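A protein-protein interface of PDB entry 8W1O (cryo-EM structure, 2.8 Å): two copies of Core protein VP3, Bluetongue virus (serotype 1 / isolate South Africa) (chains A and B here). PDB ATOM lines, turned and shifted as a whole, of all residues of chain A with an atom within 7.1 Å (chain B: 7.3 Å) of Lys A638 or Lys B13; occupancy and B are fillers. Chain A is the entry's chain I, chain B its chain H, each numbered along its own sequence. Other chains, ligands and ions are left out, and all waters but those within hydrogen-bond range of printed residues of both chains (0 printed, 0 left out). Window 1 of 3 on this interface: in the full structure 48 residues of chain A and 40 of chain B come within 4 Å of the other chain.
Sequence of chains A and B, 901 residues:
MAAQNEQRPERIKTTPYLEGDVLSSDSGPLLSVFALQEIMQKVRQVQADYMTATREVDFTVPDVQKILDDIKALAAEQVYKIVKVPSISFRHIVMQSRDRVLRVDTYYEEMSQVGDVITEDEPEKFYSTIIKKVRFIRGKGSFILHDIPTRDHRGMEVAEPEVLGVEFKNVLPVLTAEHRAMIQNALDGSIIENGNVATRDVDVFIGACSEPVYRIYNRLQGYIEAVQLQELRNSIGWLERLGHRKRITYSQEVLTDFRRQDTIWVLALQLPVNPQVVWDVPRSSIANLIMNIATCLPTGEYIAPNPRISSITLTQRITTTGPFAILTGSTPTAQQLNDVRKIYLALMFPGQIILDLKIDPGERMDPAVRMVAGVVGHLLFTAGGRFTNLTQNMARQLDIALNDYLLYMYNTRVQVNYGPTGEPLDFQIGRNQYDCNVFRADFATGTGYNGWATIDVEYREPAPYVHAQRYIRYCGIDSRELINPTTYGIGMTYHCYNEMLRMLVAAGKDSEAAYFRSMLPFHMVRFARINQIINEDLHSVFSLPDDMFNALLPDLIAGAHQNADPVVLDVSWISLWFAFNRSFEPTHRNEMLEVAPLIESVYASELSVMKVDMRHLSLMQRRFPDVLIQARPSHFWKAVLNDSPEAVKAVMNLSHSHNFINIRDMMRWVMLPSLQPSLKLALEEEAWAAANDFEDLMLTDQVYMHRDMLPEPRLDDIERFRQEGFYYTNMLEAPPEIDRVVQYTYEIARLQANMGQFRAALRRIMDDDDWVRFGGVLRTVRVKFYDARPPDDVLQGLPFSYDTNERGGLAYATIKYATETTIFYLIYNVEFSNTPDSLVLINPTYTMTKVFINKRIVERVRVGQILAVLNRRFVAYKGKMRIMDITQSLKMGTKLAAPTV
NZ of Lys B13 lies within hydrogen-bond range of O of Leu B18 (3.5 Å).
The side-chain carboxylate (OE1) of Glu B585 lies within salt-bridge range of the side-chain amino group (NZ) of Lys B13 (3.8 Å).
O of Leu A641 sits at hydrogen-bond distance from NZ of Lys A649, 3.0 Å away.
Ile B12 touches His A635 (CD1 to NE2, 3.8 Å).
Trp A637 touches Thr B14 (CZ3 to OG1, 3.2 Å).
Lys A638 touches Lys B13 (CE to O, 3.97 Å).
Leu A641 touches Thr B14 (CD1 to O, 3.9 Å).
Lys A638 touches just one residue of chain B: Lys B13 (3.97 Å).
Of chain A, only Lys A638 comes within 4 Å of Lys B13.
Of the printed residues of chain A, Thr B14 touches Trp A637 and Leu A641.
Of the printed residues of chain B, His A635 touches Ile B12.
The nearest residue of chain B that does not touch Lys A638 is Thr B14 (4.1 Å).
Of the 15 printed residues of chain A, 4 touch a printed residue of chain B.
Printed residues of chain B that touch a printed residue of chain A: Ile B12, Lys B13 and Thr B14.
Hydrophobic or aromatic side chains of chain B within 4 Å of the printed part of chain A: Ile B12.
Among the printed residues, no Asp or Glu carboxylate lies within 4 Å of a Lys or Arg side-chain nitrogen of the other chain.
No position is printed for both chains.
Of the 4 pairs that touch across the chains among the printed residues, none has its exchanged pair printed and touching as well.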
ATOM      1  N   GLU A 124     -18.239 -13.777 -16.413  1.00  0.00           N
ATOM      2  CA  GLU A 124     -18.669 -12.388 -16.296  1.00  0.00           C
ATOM      3  C   GLU A 124     -19.352 -11.907 -17.569  1.00  0.00           C
ATOM      4  O   GLU A 124     -20.370 -11.206 -17.510  1.00  0.00           O
ATOM      5  CB  GLU A 124     -17.473 -11.503 -15.968  1.00  0.00           C
ATOM      6  CG  GLU A 124     -17.820 -10.259 -15.187  1.00  0.00           C
ATOM      7  CD  GLU A 124     -16.593  -9.572 -14.640  1.00  0.00           C
ATOM      8  OE1 GLU A 124     -16.671  -9.022 -13.527  1.00  0.00           O
ATOM      9  OE2 GLU A 124     -15.550  -9.581 -15.324  1.00  0.00           O
ATOM     10  N   SER A 128     -23.176 -10.564 -18.039  1.00  0.00           N
ATOM     11  CA  SER A 128     -23.439  -9.289 -18.698  1.00  0.00           C
ATOM     12  C   SER A 128     -24.385  -9.456 -19.881  1.00  0.00           C
ATOM     13  O   SER A 128     -25.272  -8.622 -20.097  1.00  0.00           O
ATOM     14  CB  SER A 128     -22.124  -8.656 -19.148  1.00  0.00           C
ATOM     15  OG  SER A 128     -21.266  -8.440 -18.044  1.00  0.00           O
ATOM     16  N   MET A 614     -29.703  -9.222  -8.610  1.00  0.00           N
ATOM     17  CA  MET A 614     -28.814 -10.214  -8.012  1.00  0.00           C
ATOM     18  C   MET A 614     -29.585 -11.435  -7.520  1.00  0.00           C
ATOM     19  O   MET A 614     -29.080 -12.564  -7.613  1.00  0.00           O
ATOM     20  CB  MET A 614     -28.008  -9.566  -6.890  1.00  0.00           C
ATOM     21  CG  MET A 614     -27.053  -8.517  -7.432  1.00  0.00           C
ATOM     22  SD  MET A 614     -26.087  -7.606  -6.228  1.00  0.00           S
ATOM     23  CE  MET A 614     -24.979  -8.890  -5.701  1.00  0.00           C
ATOM     24  N   PRO A 633     -19.519 -16.323  -6.932  1.00  0.00           N
ATOM     25  CA  PRO A 633     -20.511 -15.253  -6.723  1.00  0.00           C
ATOM     26  C   PRO A 633     -19.989 -13.854  -7.006  1.00  0.00           C
ATOM     27  O   PRO A 633     -20.765 -12.980  -7.430  1.00  0.00           O
ATOM     28  CB  PRO A 633     -20.894 -15.423  -5.247  1.00  0.00           C
ATOM     29  CG  PRO A 633     -20.644 -16.855  -4.965  1.00  0.00           C
ATOM     30  CD  PRO A 633     -19.433 -17.223  -5.768  1.00  0.00           C
ATOM     31  N   SER A 634     -18.695 -13.614  -6.789  1.00  0.00           N
ATOM     32  CA  SER A 634     -18.127 -12.303  -7.065  1.00  0.00           C
ATOM     33  C   SER A 634     -18.223 -11.934  -8.538  1.00  0.00           C
ATOM     34  O   SER A 634     -18.244 -10.744  -8.860  1.00  0.00           O
ATOM     35  CB  SER A 634     -16.669 -12.253  -6.603  1.00  0.00           C
ATOM     36  OG  SER A 634     -15.934 -13.356  -7.099  1.00  0.00           O
ATOM     37  N   HIS A 635     -18.329 -12.920  -9.430  1.00  0.00           N
ATOM     38  CA  HIS A 635     -18.458 -12.627 -10.854  1.00  0.00           C
ATOM     39  C   HIS A 635     -19.758 -11.888 -11.156  1.00  0.00           C
ATOM     40  O   HIS A 635     -19.746 -10.814 -11.773  1.00  0.00           O
ATOM     41  CB  HIS A 635     -18.366 -13.922 -11.660  1.00  0.00           C
ATOM     42  CG  HIS A 635     -16.976 -14.466 -11.766  1.00  0.00           C
ATOM     43  ND1 HIS A 635     -16.646 -15.746 -11.379  1.00  0.00           N
ATOM     44  CD2 HIS A 635     -15.831 -13.905 -12.220  1.00  0.00           C
ATOM     45  CE1 HIS A 635     -15.358 -15.950 -11.587  1.00  0.00           C
ATOM     46  NE2 HIS A 635     -14.840 -14.847 -12.095  1.00  0.00           N
ATOM     47  N   PHE A 636     -20.896 -12.428 -10.711  1.00  0.00           N
ATOM     48  CA  PHE A 636     -22.138 -11.711 -10.971  1.00  0.00           C
ATOM     49  C   PHE A 636     -22.321 -10.515 -10.048  1.00  0.00           C
ATOM     50  O   PHE A 636     -23.020  -9.567 -10.428  1.00  0.00           O
ATOM     51  CB  PHE A 636     -23.355 -12.656 -10.928  1.00  0.00           C
ATOM     52  CG  PHE A 636     -23.656 -13.265  -9.580  1.00  0.00           C
ATOM     53  CD1 PHE A 636     -24.300 -12.542  -8.588  1.00  0.00           C
ATOM     54  CD2 PHE A 636     -23.366 -14.594  -9.339  1.00  0.00           C
ATOM     55  CE1 PHE A 636     -24.594 -13.118  -7.369  1.00  0.00           C
ATOM     56  CE2 PHE A 636     -23.668 -15.175  -8.126  1.00  0.00           C
ATOM     57  CZ  PHE A 636     -24.278 -14.437  -7.140  1.00  0.00           C
ATOM     58  N   TRP A 637     -21.682 -10.511  -8.874  1.00  0.00           N
ATOM     59  CA  TRP A 637     -21.618  -9.283  -8.086  1.00  0.00           C
ATOM     60  C   TRP A 637     -20.976  -8.155  -8.891  1.00  0.00           C
ATOM     61  O   TRP A 637     -21.520  -7.046  -8.980  1.00  0.00           O
ATOM     62  CB  TRP A 637     -20.843  -9.532  -6.791  1.00  0.00           C
ATOM     63  CG  TRP A 637     -20.916  -8.412  -5.791  1.00  0.00           C
ATOM     64  CD1 TRP A 637     -21.646  -7.265  -5.891  1.00  0.00           C
ATOM     65  CD2 TRP A 637     -20.223  -8.335  -4.538  1.00  0.00           C
ATOM     66  NE1 TRP A 637     -21.453  -6.481  -4.783  1.00  0.00           N
ATOM     67  CE2 TRP A 637     -20.584  -7.115  -3.935  1.00  0.00           C
ATOM     68  CE3 TRP A 637     -19.335  -9.182  -3.867  1.00  0.00           C
ATOM     69  CZ2 TRP A 637     -20.089  -6.719  -2.697  1.00  0.00           C
ATOM     70  CZ3 TRP A 637     -18.846  -8.787  -2.636  1.00  0.00           C
ATOM     71  CH2 TRP A 637     -19.223  -7.567  -2.064  1.00  0.00           C
ATOM     72  N   LYS A 638     -19.828  -8.436  -9.511  1.00  0.00           N
ATOM     73  CA  LYS A 638     -19.137  -7.433 -10.311  1.00  0.00           C
ATOM     74  C   LYS A 638     -19.938  -7.057 -11.550  1.00  0.00           C
ATOM     75  O   LYS A 638     -19.939  -5.891 -11.959  1.00  0.00           O
ATOM     76  CB  LYS A 638     -17.752  -7.947 -10.699  1.00  0.00           C
ATOM     77  CG  LYS A 638     -16.797  -6.874 -11.189  1.00  0.00           C
ATOM     78  CD  LYS A 638     -16.286  -6.011 -10.054  1.00  0.00           C
ATOM     79  CE  LYS A 638     -15.179  -5.087 -10.531  1.00  0.00           C
ATOM     80  NZ  LYS A 638     -15.711  -3.887 -11.231  1.00  0.00           N
ATOM     81  N   ALA A 639     -20.623  -8.024 -12.165  1.00  0.00           N
ATOM     82  CA  ALA A 639     -21.449  -7.716 -13.332  1.00  0.00           C
ATOM     83  C   ALA A 639     -22.577  -6.749 -12.977  1.00  0.00           C
ATOM     84  O   ALA A 639     -22.801  -5.748 -13.675  1.00  0.00           O
ATOM     85  CB  ALA A 639     -22.012  -9.005 -13.928  1.00  0.00           C
ATOM     86  N   VAL A 640     -23.285  -7.021 -11.878  1.00  0.00           N
ATOM     87  CA  VAL A 640     -24.377  -6.145 -11.464  1.00  0.00           C
ATOM     88  C   VAL A 640     -23.843  -4.775 -11.065  1.00  0.00           C
ATOM     89  O   VAL A 640     -24.469  -3.745 -11.344  1.00  0.00           O
ATOM     90  CB  VAL A 640     -25.188  -6.802 -10.331  1.00  0.00           C
ATOM     91  CG1 VAL A 640     -26.205  -5.834  -9.761  1.00  0.00           C
ATOM     92  CG2 VAL A 640     -25.886  -8.040 -10.849  1.00  0.00           C
ATOM     93  N   LEU A 641     -22.670  -4.734 -10.424  1.00  0.00           N
ATOM     94  CA  LEU A 641     -22.058  -3.447 -10.104  1.00  0.00           C
ATOM     95  C   LEU A 641     -21.716  -2.668 -11.368  1.00  0.00           C
ATOM     96  O   LEU A 641     -21.879  -1.444 -11.416  1.00  0.00           O
ATOM     97  CB  LEU A 641     -20.810  -3.653  -9.249  1.00  0.00           C
ATOM     98  CG  LEU A 641     -21.022  -3.917  -7.760  1.00  0.00           C
ATOM     99  CD1 LEU A 641     -19.748  -4.450  -7.135  1.00  0.00           C
ATOM    100  CD2 LEU A 641     -21.486  -2.658  -7.055  1.00  0.00           C
ATOM    101  N   ASN A 642     -21.231  -3.361 -12.401  1.00  0.00           N
ATOM    102  CA  ASN A 642     -20.912  -2.701 -13.661  1.00  0.00           C
ATOM    103  C   ASN A 642     -22.158  -2.190 -14.367  1.00  0.00           C
ATOM    104  O   ASN A 642     -22.082  -1.218 -15.126  1.00  0.00           O
ATOM    105  CB  ASN A 642     -20.148  -3.654 -14.579  1.00  0.00           C
ATOM    106  CG  ASN A 642     -18.662  -3.662 -14.304  1.00  0.00           C
ATOM    107  OD1 ASN A 642     -18.161  -2.858 -13.519  1.00  0.00           O
ATOM    108  ND2 ASN A 642     -17.946  -4.572 -14.949  1.00  0.00           N
ATOM    109  N   ASP A 643     -23.307  -2.824 -14.143  1.00  0.00           N
ATOM    110  CA  ASP A 643     -24.558  -2.378 -14.757  1.00  0.00           C
ATOM    111  C   ASP A 643     -25.395  -1.518 -13.815  1.00  0.00           C
ATOM    112  O   ASP A 643     -26.625  -1.591 -13.829  1.00  0.00           O
ATOM    113  CB  ASP A 643     -25.363  -3.575 -15.248  1.00  0.00           C
ATOM    114  CG  ASP A 643     -24.713  -4.262 -16.425  1.00  0.00           C
ATOM    115  OD1 ASP A 643     -24.010  -3.577 -17.197  1.00  0.00           O
ATOM    116  OD2 ASP A 643     -24.897  -5.486 -16.582  1.00  0.00           O
ATOM    117  N   LYS A 649     -23.343   3.642  -6.115  1.00  0.00           N
ATOM    118  CA  LYS A 649     -22.108   2.979  -5.720  1.00  0.00           C
ATOM    119  C   LYS A 649     -21.227   3.909  -4.899  1.00  0.00           C
ATOM    120  O   LYS A 649     -20.555   3.469  -3.963  1.00  0.00           O
ATOM    121  CB  LYS A 649     -21.364   2.478  -6.956  1.00  0.00           C
ATOM    122  CG  LYS A 649     -22.040   1.306  -7.650  1.00  0.00           C
ATOM    123  CD  LYS A 649     -21.181   0.754  -8.775  1.00  0.00           C
ATOM    124  CE  LYS A 649     -21.133   1.703  -9.959  1.00  0.00           C
ATOM    125  NZ  LYS A 649     -20.335   1.147 -11.085  1.00  0.00           N
ATOM    126  N   PRO B   9      -9.708 -15.870  -9.507  1.00  0.00           N
ATOM    127  CA  PRO B   9     -10.824 -15.280  -8.747  1.00  0.00           C
ATOM    128  C   PRO B   9     -10.415 -14.628  -7.436  1.00  0.00           C
ATOM    129  O   PRO B   9     -11.156 -13.775  -6.934  1.00  0.00           O
ATOM    130  CB  PRO B   9     -11.760 -16.475  -8.510  1.00  0.00           C
ATOM    131  CG  PRO B   9     -10.898 -17.679  -8.669  1.00  0.00           C
ATOM    132  CD  PRO B   9      -9.862 -17.323  -9.686  1.00  0.00           C
ATOM    133  N   GLU B  10      -9.263 -14.986  -6.864  1.00  0.00           N
ATOM    134  CA  GLU B  10      -8.861 -14.368  -5.605  1.00  0.00           C
ATOM    135  C   GLU B  10      -8.283 -12.971  -5.791  1.00  0.00           C
ATOM    136  O   GLU B  10      -8.064 -12.276  -4.794  1.00  0.00           O
ATOM    137  CB  GLU B  10      -7.845 -15.247  -4.866  1.00  0.00           C
ATOM    138  CG  GLU B  10      -6.473 -15.349  -5.516  1.00  0.00           C
ATOM    139  CD  GLU B  10      -6.391 -16.418  -6.590  1.00  0.00           C
ATOM    140  OE1 GLU B  10      -7.446 -16.894  -7.059  1.00  0.00           O
ATOM    141  OE2 GLU B  10      -5.258 -16.784  -6.967  1.00  0.00           O
ATOM    142  N   ARG B  11      -8.035 -12.544  -7.026  1.00  0.00           N
ATOM    143  CA  ARG B  11      -7.542 -11.202  -7.301  1.00  0.00           C
ATOM    144  C   ARG B  11      -8.654 -10.215  -7.629  1.00  0.00           C
ATOM    145  O   ARG B  11      -8.360  -9.059  -7.948  1.00  0.00           O
ATOM    146  CB  ARG B  11      -6.535 -11.231  -8.454  1.00  0.00           C
ATOM    147  CG  ARG B  11      -5.235 -11.947  -8.139  1.00  0.00           C
ATOM    148  CD  ARG B  11      -4.311 -11.918  -9.344  1.00  0.00           C
ATOM    149  NE  ARG B  11      -3.053 -12.612  -9.099  1.00  0.00           N
ATOM    150  CZ  ARG B  11      -2.102 -12.775 -10.009  1.00  0.00           C
ATOM    151  NH1 ARG B  11      -2.230 -12.296 -11.236  1.00  0.00           N
ATOM    152  NH2 ARG B  11      -0.996 -13.436  -9.681  1.00  0.00           N
ATOM    153  N   ILE B  12      -9.911 -10.639  -7.567  1.00  0.00           N
ATOM    154  CA  ILE B  12     -11.036  -9.761  -7.868  1.00  0.00           C
ATOM    155  C   ILE B  12     -11.389  -8.949  -6.631  1.00  0.00           C
ATOM    156  O   ILE B  12     -11.550  -9.496  -5.534  1.00  0.00           O
ATOM    157  CB  ILE B  12     -12.241 -10.582  -8.362  1.00  0.00           C
ATOM    158  CG1 ILE B  12     -11.961 -11.163  -9.747  1.00  0.00           C
ATOM    159  CG2 ILE B  12     -13.497  -9.729  -8.395  1.00  0.00           C
ATOM    160  CD1 ILE B  12     -12.917 -12.261 -10.146  1.00  0.00           C
ATOM    161  N   LYS B  13     -11.509  -7.634  -6.803  1.00  0.00           N
ATOM    162  CA  LYS B  13     -11.867  -6.731  -5.716  1.00  0.00           C
ATOM    163  C   LYS B  13     -13.167  -6.027  -6.072  1.00  0.00           C
ATOM    164  O   LYS B  13     -13.236  -5.317  -7.080  1.00  0.00           O
ATOM    165  CB  LYS B  13     -10.752  -5.717  -5.453  1.00  0.00           C
ATOM    166  CG  LYS B  13      -9.465  -6.349  -4.953  1.00  0.00           C
ATOM    167  CD  LYS B  13      -8.353  -5.327  -4.815  1.00  0.00           C
ATOM    168  CE  LYS B  13      -7.007  -6.011  -4.633  1.00  0.00           C
ATOM    169  NZ  LYS B  13      -5.894  -5.032  -4.500  1.00  0.00           N
ATOM    170  N   THR B  14     -14.192  -6.224  -5.242  1.00  0.00           N
ATOM    171  CA  THR B  14     -15.504  -5.631  -5.463  1.00  0.00           C
ATOM    172  C   THR B  14     -15.767  -4.405  -4.598  1.00  0.00           C
ATOM    173  O   THR B  14     -16.710  -3.659  -4.882  1.00  0.00           O
ATOM    174  CB  THR B  14     -16.603  -6.667  -5.207  1.00  0.00           C
ATOM    175  OG1 THR B  14     -16.322  -7.370  -3.991  1.00  0.00           O
ATOM    176  CG2 THR B  14     -16.675  -7.663  -6.353  1.00  0.00           C
ATOM    177  N   THR B  15     -14.969  -4.184  -3.564  1.00  0.00           N
ATOM    178  CA  THR B  15     -15.059  -3.024  -2.694  1.00  0.00           C
ATOM    179  C   THR B  15     -13.689  -2.373  -2.615  1.00  0.00           C
ATOM    180  O   THR B  15     -12.664  -3.053  -2.740  1.00  0.00           O
ATOM    181  CB  THR B  15     -15.541  -3.415  -1.287  1.00  0.00           C
ATOM    182  OG1 THR B  15     -14.767  -4.516  -0.800  1.00  0.00           O
ATOM    183  CG2 THR B  15     -17.006  -3.808  -1.317  1.00  0.00           C
ATOM    184  N   PRO B  16     -13.630  -1.056  -2.407  1.00  0.00           N
ATOM    185  CA  PRO B  16     -12.343  -0.354  -2.413  1.00  0.00           C
ATOM    186  C   PRO B  16     -11.557  -0.433  -1.113  1.00  0.00           C
ATOM    187  O   PRO B  16     -10.606   0.336  -0.949  1.00  0.00           O
ATOM    188  CB  PRO B  16     -12.761   1.095  -2.700  1.00  0.00           C
ATOM    189  CG  PRO B  16     -14.092   1.211  -2.085  1.00  0.00           C
ATOM    190  CD  PRO B  16     -14.762  -0.118  -2.288  1.00  0.00           C
ATOM    191  N   TYR B  17     -11.923  -1.322  -0.187  1.00  0.00           N
ATOM    192  CA  TYR B  17     -11.175  -1.444   1.061  1.00  0.00           C
ATOM    193  C   TYR B  17      -9.741  -1.895   0.808  1.00  0.00           C
ATOM    194  O   TYR B  17      -8.799  -1.353   1.397  1.00  0.00           O
ATOM    195  CB  TYR B  17     -11.890  -2.414   2.002  1.00  0.00           C
ATOM    196  CG  TYR B  17     -11.199  -2.642   3.329  1.00  0.00           C
ATOM    197  CD1 TYR B  17     -11.444  -1.814   4.412  1.00  0.00           C
ATOM    198  CD2 TYR B  17     -10.317  -3.702   3.504  1.00  0.00           C
ATOM    199  CE1 TYR B  17     -10.824  -2.023   5.626  1.00  0.00           C
ATOM    200  CE2 TYR B  17      -9.691  -3.916   4.713  1.00  0.00           C
ATOM    201  CZ  TYR B  17      -9.947  -3.073   5.770  1.00  0.00           C
ATOM    202  OH  TYR B  17      -9.330  -3.285   6.978  1.00  0.00           O
ATOM    203  N   LEU B  18      -9.553  -2.874  -0.072  1.00  0.00           N
ATOM    204  CA  LEU B  18      -8.234  -3.435  -0.332  1.00  0.00           C
ATOM    205  C   LEU B  18      -7.446  -2.652  -1.372  1.00  0.00           C
ATOM    206  O   LEU B  18      -6.308  -3.023  -1.672  1.00  0.00           O
ATOM    207  CB  LEU B  18      -8.361  -4.895  -0.773  1.00  0.00           C
ATOM    208  CG  LEU B  18      -8.830  -5.876   0.301  1.00  0.00           C
ATOM    209  CD1 LEU B  18      -9.172  -7.220  -0.316  1.00  0.00           C
ATOM    210  CD2 LEU B  18      -7.778  -6.035   1.384  1.00  0.00           C
ATOM    211  N   GLU B  19      -8.016  -1.587  -1.925  1.00  0.00           N
ATOM    212  CA  GLU B  19      -7.299  -0.774  -2.894  1.00  0.00           C
ATOM    213  C   GLU B  19      -6.244   0.084  -2.204  1.00  0.00           C
ATOM    214  O   GLU B  19      -6.486   0.664  -1.144  1.00  0.00           O
ATOM    215  CB  GLU B  19      -8.280   0.113  -3.661  1.00  0.00           C
ATOM    216  CG  GLU B  19      -7.648   0.983  -4.738  1.00  0.00           C
ATOM    217  CD  GLU B  19      -7.045   0.180  -5.875  1.00  0.00           C
ATOM    218  OE1 GLU B  19      -7.497  -0.958  -6.115  1.00  0.00           O
ATOM    219  OE2 GLU B  19      -6.117   0.695  -6.534  1.00  0.00           O
ATOM    220  N   GLY B  20      -5.067   0.161  -2.816  1.00  0.00           N
ATOM    221  CA  GLY B  20      -3.988   0.977  -2.289  1.00  0.00           C
ATOM    222  C   GLY B  20      -2.983   1.264  -3.380  1.00  0.00           C
ATOM    223  O   GLY B  20      -3.048   0.707  -4.478  1.00  0.00           O
ATOM    224  N   ILE B 303       1.826  -2.946  -1.389  1.00  0.00           N
ATOM    225  CA  ILE B 303       0.638  -2.102  -1.423  1.00  0.00           C
ATOM    226  C   ILE B 303       0.396  -1.529  -0.034  1.00  0.00           C
ATOM    227  O   ILE B 303       0.428  -2.258   0.963  1.00  0.00           O
ATOM    228  CB  ILE B 303      -0.599  -2.887  -1.906  1.00  0.00           C
ATOM    229  CG1 ILE B 303      -0.299  -3.622  -3.211  1.00  0.00           C
ATOM    230  CG2 ILE B 303      -1.781  -1.957  -2.090  1.00  0.00           C
ATOM    231  CD1 ILE B 303       0.049  -2.712  -4.361  1.00  0.00           C
ATOM    232  N   ARG B 529      -2.402 -14.245   1.676  1.00  0.00           N
ATOM    233  CA  ARG B 529      -1.557 -14.203   0.484  1.00  0.00           C
ATOM    234  C   ARG B 529      -0.199 -14.848   0.742  1.00  0.00           C
ATOM    235  O   ARG B 529       0.334 -15.564  -0.119  1.00  0.00           O
ATOM    236  CB  ARG B 529      -1.388 -12.760   0.010  1.00  0.00           C
ATOM    237  CG  ARG B 529      -2.679 -12.106  -0.443  1.00  0.00           C
ATOM    238  CD  ARG B 529      -2.414 -11.013  -1.465  1.00  0.00           C
ATOM    239  NE  ARG B 529      -3.464 -10.000  -1.504  1.00  0.00           N
ATOM    240  CZ  ARG B 529      -4.687 -10.190  -1.985  1.00  0.00           C
ATOM    241  NH1 ARG B 529      -5.062 -11.357  -2.485  1.00  0.00           N
ATOM    242  NH2 ARG B 529      -5.553  -9.182  -1.969  1.00  0.00           N
ATOM    243  N   GLU B 585       1.968  -8.491  -2.880  1.00  0.00           N
ATOM    244  CA  GLU B 585       0.981  -9.040  -3.806  1.00  0.00           C
ATOM    245  C   GLU B 585       1.681  -9.449  -5.094  1.00  0.00           C
ATOM    246  O   GLU B 585       2.181  -8.573  -5.827  1.00  0.00           O
ATOM    247  CB  GLU B 585      -0.122  -8.021  -4.093  1.00  0.00           C
ATOM    248  CG  GLU B 585      -0.905  -7.583  -2.873  1.00  0.00           C
ATOM    249  CD  GLU B 585      -2.164  -6.828  -3.238  1.00  0.00           C
ATOM    250  OE1 GLU B 585      -2.402  -6.623  -4.446  1.00  0.00           O
ATOM    251  OE2 GLU B 585      -2.911  -6.434  -2.319  1.00  0.00           O
